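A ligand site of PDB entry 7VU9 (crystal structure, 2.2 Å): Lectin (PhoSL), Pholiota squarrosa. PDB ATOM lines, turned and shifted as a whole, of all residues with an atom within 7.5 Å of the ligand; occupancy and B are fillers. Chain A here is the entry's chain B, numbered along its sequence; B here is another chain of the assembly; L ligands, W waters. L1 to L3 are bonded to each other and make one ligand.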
ATOM      1  N   CYS A  10     -22.674 -34.047 -12.031  1.00  0.00           N
ATOM      2  CA  CYS A  10     -23.251 -32.690 -11.955  1.00  0.00           C
ATOM      3  C   CYS A  10     -23.863 -32.365 -13.331  1.00  0.00           C
ATOM      4  O   CYS A  10     -23.443 -32.960 -14.324  1.00  0.00           O
ATOM      5  CB  CYS A  10     -22.252 -31.698 -11.376  1.00  0.00           C
ATOM      6  SG  CYS A  10     -21.578 -32.201  -9.751  1.00  0.00           S
ATOM      7  N   ASP A  11     -24.870 -31.515 -13.333  1.00  0.00           N
ATOM      8  CA  ASP A  11     -25.596 -31.115 -14.557  1.00  0.00           C
ATOM      9  C   ASP A  11     -25.572 -29.580 -14.658  1.00  0.00           C
ATOM     10  O   ASP A  11     -26.178 -28.899 -13.797  1.00  0.00           O
ATOM     11  CB  ASP A  11     -26.995 -31.718 -14.579  1.00  0.00           C
ATOM     12  CG  ASP A  11     -27.676 -31.605 -15.944  1.00  0.00           C
ATOM     13  OD1 ASP A  11     -27.439 -30.600 -16.671  1.00  0.00           O
ATOM     14  OD2 ASP A  11     -28.434 -32.532 -16.274  1.00  0.00           O
ATOM     15  N   GLY A  12     -24.897 -29.053 -15.670  1.00  0.00           N
ATOM     16  CA  GLY A  12     -24.825 -27.602 -15.919  1.00  0.00           C
ATOM     17  C   GLY A  12     -26.069 -27.041 -16.610  1.00  0.00           C
ATOM     18  O   GLY A  12     -26.070 -25.844 -16.864  1.00  0.00           O
ATOM     19  N   ASP A  13     -27.092 -27.837 -16.888  1.00  0.00           N
ATOM     20  CA  ASP A  13     -28.395 -27.296 -17.386  1.00  0.00           C
ATOM     21  C   ASP A  13     -29.337 -27.094 -16.182  1.00  0.00           C
ATOM     22  O   ASP A  13     -30.053 -26.064 -16.123  1.00  0.00           O
ATOM     23  CB  ASP A  13     -28.954 -28.187 -18.504  1.00  0.00           C
ATOM     24  CG  ASP A  13     -28.170 -28.138 -19.812  1.00  0.00           C
ATOM     25  OD1 ASP A  13     -27.954 -27.038 -20.348  1.00  0.00           O
ATOM     26  OD2 ASP A  13     -27.742 -29.209 -20.276  1.00  0.00           O
ATOM     27  N   THR A  14     -29.314 -27.997 -15.205  1.00  0.00           N
ATOM     28  CA  THR A  14     -30.227 -28.000 -14.025  1.00  0.00           C
ATOM     29  C   THR A  14     -29.546 -27.401 -12.787  1.00  0.00           C
ATOM     30  O   THR A  14     -30.255 -27.107 -11.824  1.00  0.00           O
ATOM     31  CB  THR A  14     -30.690 -29.436 -13.755  1.00  0.00           C
ATOM     32  OG1 THR A  14     -29.551 -30.230 -13.369  1.00  0.00           O
ATOM     33  CG2 THR A  14     -31.339 -30.086 -14.958  1.00  0.00           C
ATOM     34  N   TYR A  15     -28.214 -27.287 -12.805  1.00  0.00           N
ATOM     35  CA  TYR A  15     -27.374 -26.748 -11.693  1.00  0.00           C
ATOM     36  C   TYR A  15     -27.594 -27.557 -10.413  1.00  0.00           C
ATOM     37  O   TYR A  15     -27.761 -27.004  -9.315  1.00  0.00           O
ATOM     38  CB  TYR A  15     -27.659 -25.261 -11.487  1.00  0.00           C
ATOM     39  CG  TYR A  15     -27.231 -24.446 -12.670  1.00  0.00           C
ATOM     40  CD1 TYR A  15     -28.046 -24.322 -13.796  1.00  0.00           C
ATOM     41  CD2 TYR A  15     -25.994 -23.842 -12.708  1.00  0.00           C
ATOM     42  CE1 TYR A  15     -27.640 -23.581 -14.891  1.00  0.00           C
ATOM     43  CE2 TYR A  15     -25.569 -23.092 -13.789  1.00  0.00           C
ATOM     44  CZ  TYR A  15     -26.398 -22.972 -14.888  1.00  0.00           C
ATOM     45  OH  TYR A  15     -25.967 -22.239 -15.938  1.00  0.00           O
ATOM     46  N   ALA A  35     -23.467 -23.966  -7.974  1.00  0.00           N
ATOM     47  CA  ALA A  35     -22.978 -23.130  -9.086  1.00  0.00           C
ATOM     48  C   ALA A  35     -22.215 -24.071 -10.033  1.00  0.00           C
ATOM     49  O   ALA A  35     -21.584 -25.001  -9.549  1.00  0.00           O
ATOM     50  CB  ALA A  35     -22.127 -22.000  -8.594  1.00  0.00           C
ATOM     51  N   VAL A  36     -22.348 -23.837 -11.338  1.00  0.00           N
ATOM     52  CA  VAL A  36     -21.573 -24.512 -12.409  1.00  0.00           C
ATOM     53  C   VAL A  36     -21.048 -23.400 -13.291  1.00  0.00           C
ATOM     54  O   VAL A  36     -21.854 -22.561 -13.716  1.00  0.00           O
ATOM     55  CB  VAL A  36     -22.398 -25.523 -13.230  1.00  0.00           C
ATOM     56  CG1 VAL A  36     -21.570 -26.207 -14.297  1.00  0.00           C
ATOM     57  CG2 VAL A  36     -23.072 -26.558 -12.365  1.00  0.00           C
ATOM     58  N   PHE A  37     -19.757 -23.414 -13.528  1.00  0.00           N
ATOM     59  CA  PHE A  37     -19.120 -22.389 -14.368  1.00  0.00           C
ATOM     60  C   PHE A  37     -17.797 -22.902 -14.925  1.00  0.00           C
ATOM     61  O   PHE A  37     -17.225 -23.870 -14.426  1.00  0.00           O
ATOM     62  CB  PHE A  37     -18.938 -21.081 -13.610  1.00  0.00           C
ATOM     63  CG  PHE A  37     -18.302 -21.196 -12.251  1.00  0.00           C
ATOM     64  CD1 PHE A  37     -16.930 -21.343 -12.121  1.00  0.00           C
ATOM     65  CD2 PHE A  37     -19.078 -21.168 -11.102  1.00  0.00           C
ATOM     66  CE1 PHE A  37     -16.350 -21.444 -10.871  1.00  0.00           C
ATOM     67  CE2 PHE A  37     -18.488 -21.271  -9.854  1.00  0.00           C
ATOM     68  CZ  PHE A  37     -17.121 -21.379  -9.737  1.00  0.00           C
ATOM     69  N   HIS A  38     -17.326 -22.178 -15.913  1.00  0.00           N
ATOM     70  CA  HIS A  38     -16.018 -22.362 -16.557  1.00  0.00           C
ATOM     71  C   HIS A  38     -15.014 -21.507 -15.798  1.00  0.00           C
ATOM     72  O   HIS A  38     -15.397 -20.416 -15.341  1.00  0.00           O
ATOM     73  CB  HIS A  38     -16.153 -21.933 -18.007  1.00  0.00           C
ATOM     74  CG  HIS A  38     -14.941 -22.188 -18.823  1.00  0.00           C
ATOM     75  ND1 HIS A  38     -14.019 -21.198 -19.080  1.00  0.00           N
ATOM     76  CD2 HIS A  38     -14.530 -23.285 -19.481  1.00  0.00           C
ATOM     77  CE1 HIS A  38     -13.103 -21.685 -19.898  1.00  0.00           C
ATOM     78  NE2 HIS A  38     -13.389 -22.957 -20.153  1.00  0.00           N
ATOM     79  N   ALA B   1     -26.892 -31.811 -19.287  1.00  0.00           N
ATOM     80  CA  ALA B   1     -26.692 -33.288 -19.271  1.00  0.00           C
ATOM     81  C   ALA B   1     -25.801 -33.632 -18.079  1.00  0.00           C
ATOM     82  O   ALA B   1     -24.866 -32.909 -17.784  1.00  0.00           O
ATOM     83  CB  ALA B   1     -26.062 -33.763 -20.563  1.00  0.00           C
ATOM     84  N   PRO B   2     -26.076 -34.721 -17.341  1.00  0.00           N
ATOM     85  CA  PRO B   2     -25.232 -35.064 -16.196  1.00  0.00           C
ATOM     86  C   PRO B   2     -23.869 -35.502 -16.752  1.00  0.00           C
ATOM     87  O   PRO B   2     -23.812 -36.176 -17.768  1.00  0.00           O
ATOM     88  CB  PRO B   2     -25.999 -36.163 -15.462  1.00  0.00           C
ATOM     89  CG  PRO B   2     -26.889 -36.779 -16.539  1.00  0.00           C
ATOM     90  CD  PRO B   2     -27.187 -35.661 -17.522  1.00  0.00           C
ATOM     91  N   VAL B   3     -22.796 -35.031 -16.122  1.00  0.00           N
ATOM     92  CA  VAL B   3     -21.416 -35.410 -16.476  1.00  0.00           C
ATOM     93  C   VAL B   3     -20.738 -35.833 -15.189  1.00  0.00           C
ATOM     94  O   VAL B   3     -21.124 -35.396 -14.109  1.00  0.00           O
ATOM     95  CB  VAL B   3     -20.670 -34.284 -17.194  1.00  0.00           C
ATOM     96  CG1 VAL B   3     -21.432 -33.837 -18.430  1.00  0.00           C
ATOM     97  CG2 VAL B   3     -20.366 -33.116 -16.264  1.00  0.00           C
ATOM     98  N   LEU B  21     -15.209 -31.202 -13.354  1.00  0.00           N
ATOM     99  CA  LEU B  21     -16.154 -31.967 -14.196  1.00  0.00           C
ATOM    100  C   LEU B  21     -15.410 -32.533 -15.404  1.00  0.00           C
ATOM    101  O   LEU B  21     -14.458 -31.913 -15.884  1.00  0.00           O
ATOM    102  CB  LEU B  21     -17.300 -31.040 -14.602  1.00  0.00           C
ATOM    103  CG  LEU B  21     -18.095 -30.449 -13.432  1.00  0.00           C
ATOM    104  CD1 LEU B  21     -19.320 -29.667 -13.936  1.00  0.00           C
ATOM    105  CD2 LEU B  21     -18.544 -31.533 -12.473  1.00  0.00           C
ATOM    106  N   ASP B  22     -15.814 -33.720 -15.847  1.00  0.00           N
ATOM    107  CA  ASP B  22     -15.325 -34.393 -17.061  1.00  0.00           C
ATOM    108  C   ASP B  22     -16.221 -33.916 -18.200  1.00  0.00           C
ATOM    109  O   ASP B  22     -17.222 -34.614 -18.484  1.00  0.00           O
ATOM    110  CB  ASP B  22     -15.326 -35.926 -16.926  1.00  0.00           C
ATOM    111  CG  ASP B  22     -14.635 -36.668 -18.068  1.00  0.00           C
ATOM    112  OD1 ASP B  22     -13.928 -36.004 -18.891  1.00  0.00           O
ATOM    113  OD2 ASP B  22     -14.790 -37.913 -18.116  1.00  0.00           O
ATOM    114  N   TYR B  23     -15.891 -32.763 -18.792  1.00  0.00           N
ATOM    115  CA  TYR B  23     -16.697 -32.116 -19.850  1.00  0.00           C
ATOM    116  C   TYR B  23     -15.838 -31.108 -20.597  1.00  0.00           C
ATOM    117  O   TYR B  23     -15.062 -30.372 -19.948  1.00  0.00           O
ATOM    118  CB  TYR B  23     -17.952 -31.447 -19.267  1.00  0.00           C
ATOM    119  CG  TYR B  23     -18.782 -30.741 -20.311  1.00  0.00           C
ATOM    120  CD1 TYR B  23     -19.664 -31.430 -21.118  1.00  0.00           C
ATOM    121  CD2 TYR B  23     -18.621 -29.383 -20.520  1.00  0.00           C
ATOM    122  CE1 TYR B  23     -20.399 -30.783 -22.095  1.00  0.00           C
ATOM    123  CE2 TYR B  23     -19.328 -28.711 -21.498  1.00  0.00           C
ATOM    124  CZ  TYR B  23     -20.229 -29.414 -22.286  1.00  0.00           C
ATOM    125  OH  TYR B  23     -20.940 -28.738 -23.242  1.00  0.00           O
ATOM    126  N   GLY B  24     -16.013 -31.055 -21.925  1.00  0.00           N
ATOM    127  CA  GLY B  24     -15.421 -30.050 -22.821  1.00  0.00           C
ATOM    128  C   GLY B  24     -13.921 -29.875 -22.639  1.00  0.00           C
ATOM    129  O   GLY B  24     -13.178 -30.862 -22.647  1.00  0.00           O
ATOM    130  N   ASP B  25     -13.494 -28.626 -22.432  1.00  0.00           N
ATOM    131  CA  ASP B  25     -12.090 -28.230 -22.276  1.00  0.00           C
ATOM    132  C   ASP B  25     -11.525 -28.649 -20.907  1.00  0.00           C
ATOM    133  O   ASP B  25     -10.337 -28.355 -20.676  1.00  0.00           O
ATOM    134  CB  ASP B  25     -11.917 -26.726 -22.523  1.00  0.00           C
ATOM    135  CG  ASP B  25     -12.587 -25.821 -21.499  1.00  0.00           C
ATOM    136  OD1 ASP B  25     -13.273 -26.375 -20.598  1.00  0.00           O
ATOM    137  OD2 ASP B  25     -12.445 -24.580 -21.617  1.00  0.00           O
ATOM    138  N   TRP B  28     -14.481 -26.783 -16.496  1.00  0.00           N
ATOM    139  CA  TRP B  28     -15.781 -26.569 -15.847  1.00  0.00           C
ATOM    140  C   TRP B  28     -15.751 -27.181 -14.450  1.00  0.00           C
ATOM    141  O   TRP B  28     -15.214 -28.268 -14.292  1.00  0.00           O
ATOM    142  CB  TRP B  28     -16.887 -27.168 -16.677  1.00  0.00           C
ATOM    143  CG  TRP B  28     -16.985 -26.523 -18.010  1.00  0.00           C
ATOM    144  CD1 TRP B  28     -16.299 -26.869 -19.131  1.00  0.00           C
ATOM    145  CD2 TRP B  28     -17.870 -25.455 -18.384  1.00  0.00           C
ATOM    146  NE1 TRP B  28     -16.681 -26.063 -20.173  1.00  0.00           N
ATOM    147  CE2 TRP B  28     -17.647 -25.194 -19.744  1.00  0.00           C
ATOM    148  CE3 TRP B  28     -18.807 -24.687 -17.700  1.00  0.00           C
ATOM    149  CZ2 TRP B  28     -18.337 -24.205 -20.447  1.00  0.00           C
ATOM    150  CZ3 TRP B  28     -19.477 -23.697 -18.378  1.00  0.00           C
ATOM    151  CH2 TRP B  28     -19.240 -23.460 -19.741  1.00  0.00           C
ATOM    152  N   VAL B  29     -16.384 -26.502 -13.506  1.00  0.00           N
ATOM    153  CA  VAL B  29     -16.523 -26.936 -12.096  1.00  0.00           C
ATOM    154  C   VAL B  29     -17.952 -26.676 -11.640  1.00  0.00           C
ATOM    155  O   VAL B  29     -18.654 -25.801 -12.168  1.00  0.00           O
ATOM    156  CB  VAL B  29     -15.528 -26.228 -11.161  1.00  0.00           C
ATOM    157  CG1 VAL B  29     -14.106 -26.319 -11.662  1.00  0.00           C
ATOM    158  CG2 VAL B  29     -15.910 -24.775 -10.896  1.00  0.00           C
ATOM    159  N   ALA B  30     -18.330 -27.437 -10.638  1.00  0.00           N
ATOM    160  CA  ALA B  30     -19.513 -27.235  -9.796  1.00  0.00           C
ATOM    161  C   ALA B  30     -18.943 -26.794  -8.450  1.00  0.00           C
ATOM    162  O   ALA B  30     -17.917 -27.323  -8.078  1.00  0.00           O
ATOM    163  CB  ALA B  30     -20.290 -28.515  -9.704  1.00  0.00           C
HETATM  164  C1  LIG L   1     -24.967 -24.073 -20.942  1.00  0.00           C
HETATM  165  C2  LIG L   1     -25.322 -23.301 -19.657  1.00  0.00           C
HETATM  166  C3  LIG L   1     -26.824 -23.327 -19.341  1.00  0.00           C
HETATM  167  C4  LIG L   1     -27.617 -23.003 -20.609  1.00  0.00           C
HETATM  168  C5  LIG L   1     -27.186 -23.931 -21.748  1.00  0.00           C
HETATM  169  C6  LIG L   1     -27.995 -23.732 -23.042  1.00  0.00           C
HETATM  170  C7  LIG L   1     -23.586 -23.209 -17.942  1.00  0.00           C
HETATM  171  C8  LIG L   1     -23.104 -23.747 -16.639  1.00  0.00           C
HETATM  172  N1  LIG L   1     -24.649 -23.798 -18.458  1.00  0.00           N
HETATM  173  O1  LIG L   1     -27.150 -22.454 -18.235  1.00  0.00           O
HETATM  174  O2  LIG L   1     -29.004 -23.170 -20.333  1.00  0.00           O
HETATM  175  O3  LIG L   1     -25.789 -23.716 -22.032  1.00  0.00           O
HETATM  176  O4  LIG L   1     -28.371 -22.336 -23.201  1.00  0.00           O
HETATM  177  O5  LIG L   1     -23.063 -22.275 -18.509  1.00  0.00           O
HETATM  178  C1  LG2 L   2     -20.698 -25.332 -23.691  1.00  0.00           C
HETATM  179  C2  LG2 L   2     -22.035 -25.141 -24.423  1.00  0.00           C
HETATM  180  C3  LG2 L   2     -22.919 -24.230 -23.622  1.00  0.00           C
HETATM  181  C4  LG2 L   2     -23.064 -24.776 -22.211  1.00  0.00           C
HETATM  182  C5  LG2 L   2     -21.717 -25.135 -21.617  1.00  0.00           C
HETATM  183  C6  LG2 L   2     -21.890 -25.863 -20.287  1.00  0.00           C
HETATM  184  C7  LG2 L   2     -22.461 -25.033 -26.827  1.00  0.00           C
HETATM  185  C8  LG2 L   2     -21.886 -24.474 -28.094  1.00  0.00           C
HETATM  186  N1  LG2 L   2     -21.817 -24.595 -25.743  1.00  0.00           N
HETATM  187  O1  LG2 L   2     -19.764 -26.166 -24.400  1.00  0.00           O
HETATM  188  O2  LG2 L   2     -24.229 -24.097 -24.166  1.00  0.00           O
HETATM  189  O3  LG2 L   2     -23.631 -23.803 -21.348  1.00  0.00           O
HETATM  190  O4  LG2 L   2     -21.000 -25.996 -22.502  1.00  0.00           O
HETATM  191  O5  LG2 L   2     -22.586 -27.126 -20.450  1.00  0.00           O
HETATM  192  O6  LG2 L   2     -23.384 -25.860 -26.787  1.00  0.00           O
HETATM  193  C1  LG3 L   3     -23.520 -27.475 -19.403  1.00  0.00           C
HETATM  194  C2  LG3 L   3     -24.389 -28.619 -19.940  1.00  0.00           C
HETATM  195  C3  LG3 L   3     -23.504 -29.841 -20.160  1.00  0.00           C
HETATM  196  C4  LG3 L   3     -22.678 -30.161 -18.893  1.00  0.00           C
HETATM  197  C5  LG3 L   3     -21.899 -28.947 -18.479  1.00  0.00           C
HETATM  198  C6  LG3 L   3     -21.152 -29.260 -17.195  1.00  0.00           C
HETATM  199  O1  LG3 L   3     -25.030 -28.192 -21.155  1.00  0.00           O
HETATM  200  O2  LG3 L   3     -24.295 -30.975 -20.407  1.00  0.00           O
HETATM  201  O3  LG3 L   3     -23.585 -30.536 -17.843  1.00  0.00           O
HETATM  202  O4  LG3 L   3     -22.850 -27.885 -18.242  1.00  0.00           O
HETATM  203  O   HOH W   1     -21.128 -20.682 -19.213  1.00  0.00           O
HETATM  204  O   HOH W   2     -23.736 -28.364 -23.457  1.00  0.00           O
HETATM  205  O   HOH W   3     -23.193 -33.106 -22.031  1.00  0.00           O
HETATM  206  O   HOH W   4     -27.797 -27.186 -22.959  1.00  0.00           O
HETATM  207  O   HOH W   5     -25.232 -26.510 -25.280  1.00  0.00           O
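An oxygen (O1) of LG3 L3 is in hydrogen-bond range of the side-chain carboxylate (OD2) of Asp 13, at 3.0 Å.
An oxygen (O1) of LIG L1 is in hydrogen-bond range of the side-chain hydroxyl (OH) of Tyr 15, 2.6 Å away.
The backbone carbonyl oxygen (O) of Ala 1 of chain B is in hydrogen-bond range of an oxygen (O3) of LG3 L3 (2.7 Å).
An oxygen (O2) of LG3 L3 sits at hydrogen-bond distance from the backbone NH of Ala 1 of chain B (2.9 Å).
O of Gly 12 lies within hydrogen-bond range of N1 of LIG L1 (3.0 Å).
N of Gly 12 is in hydrogen-bond range of O3 of LG3 L3 (2.9 Å).
The side-chain hydroxyl (OH) of Tyr 23 of chain B sits at hydrogen-bond distance from an oxygen (O4) of LG2 L2 (2.8 Å).
OD1 of Asp 11 lies within hydrogen-bond range of N of Asp 13, at 2.8 Å.
The backbone NH (N) of Val 3 of chain B lies within hydrogen-bond range of the backbone carbonyl oxygen (O) of Cys 10 (2.8 Å).
N of Ala 1 of chain B is in hydrogen-bond range of OD1 of Asp 11, 2.9 Å away.
O of Trp 28 of chain B is in hydrogen-bond range of N of Leu 21 of chain B (3.1 Å).
The indole nitrogen of Trp 28 of chain B sits close to the side-chain carboxylate of Asp 25 of chain B (3.4 Å).
N of Ala 1 of chain B is in hydrogen-bond range of OD2 of Asp 13, at 2.9 Å.
Merely in contact with the ligand: Asp 11 (3.9 Å), Val 36 (3.4 Å), Val 3 of chain B (3.9 Å), Leu 21 of chain B (3.8 Å) and Trp 28 of chain B (3.5 Å).
Hydrophobic or aromatic side chains within 4 Å of the ligand: Tyr 15, Val 36, Ala 1 of chain B, Val 3 of chain B, Leu 21 of chain B, Tyr 23 of chain B and Trp 28 of chain B.
Of the 21 residues printed, 10 come within 4 Å of the ligand.
Water W2 lies within hydrogen-bond range of O1 of LG3 L3 (2.6 Å) and OH of Tyr 23 of chain B (2.8 Å).
Water W4 lies within hydrogen-bond range of OD1 of Asp 13 (2.6 Å) and O1 of LG3 L3 (3.5 Å).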
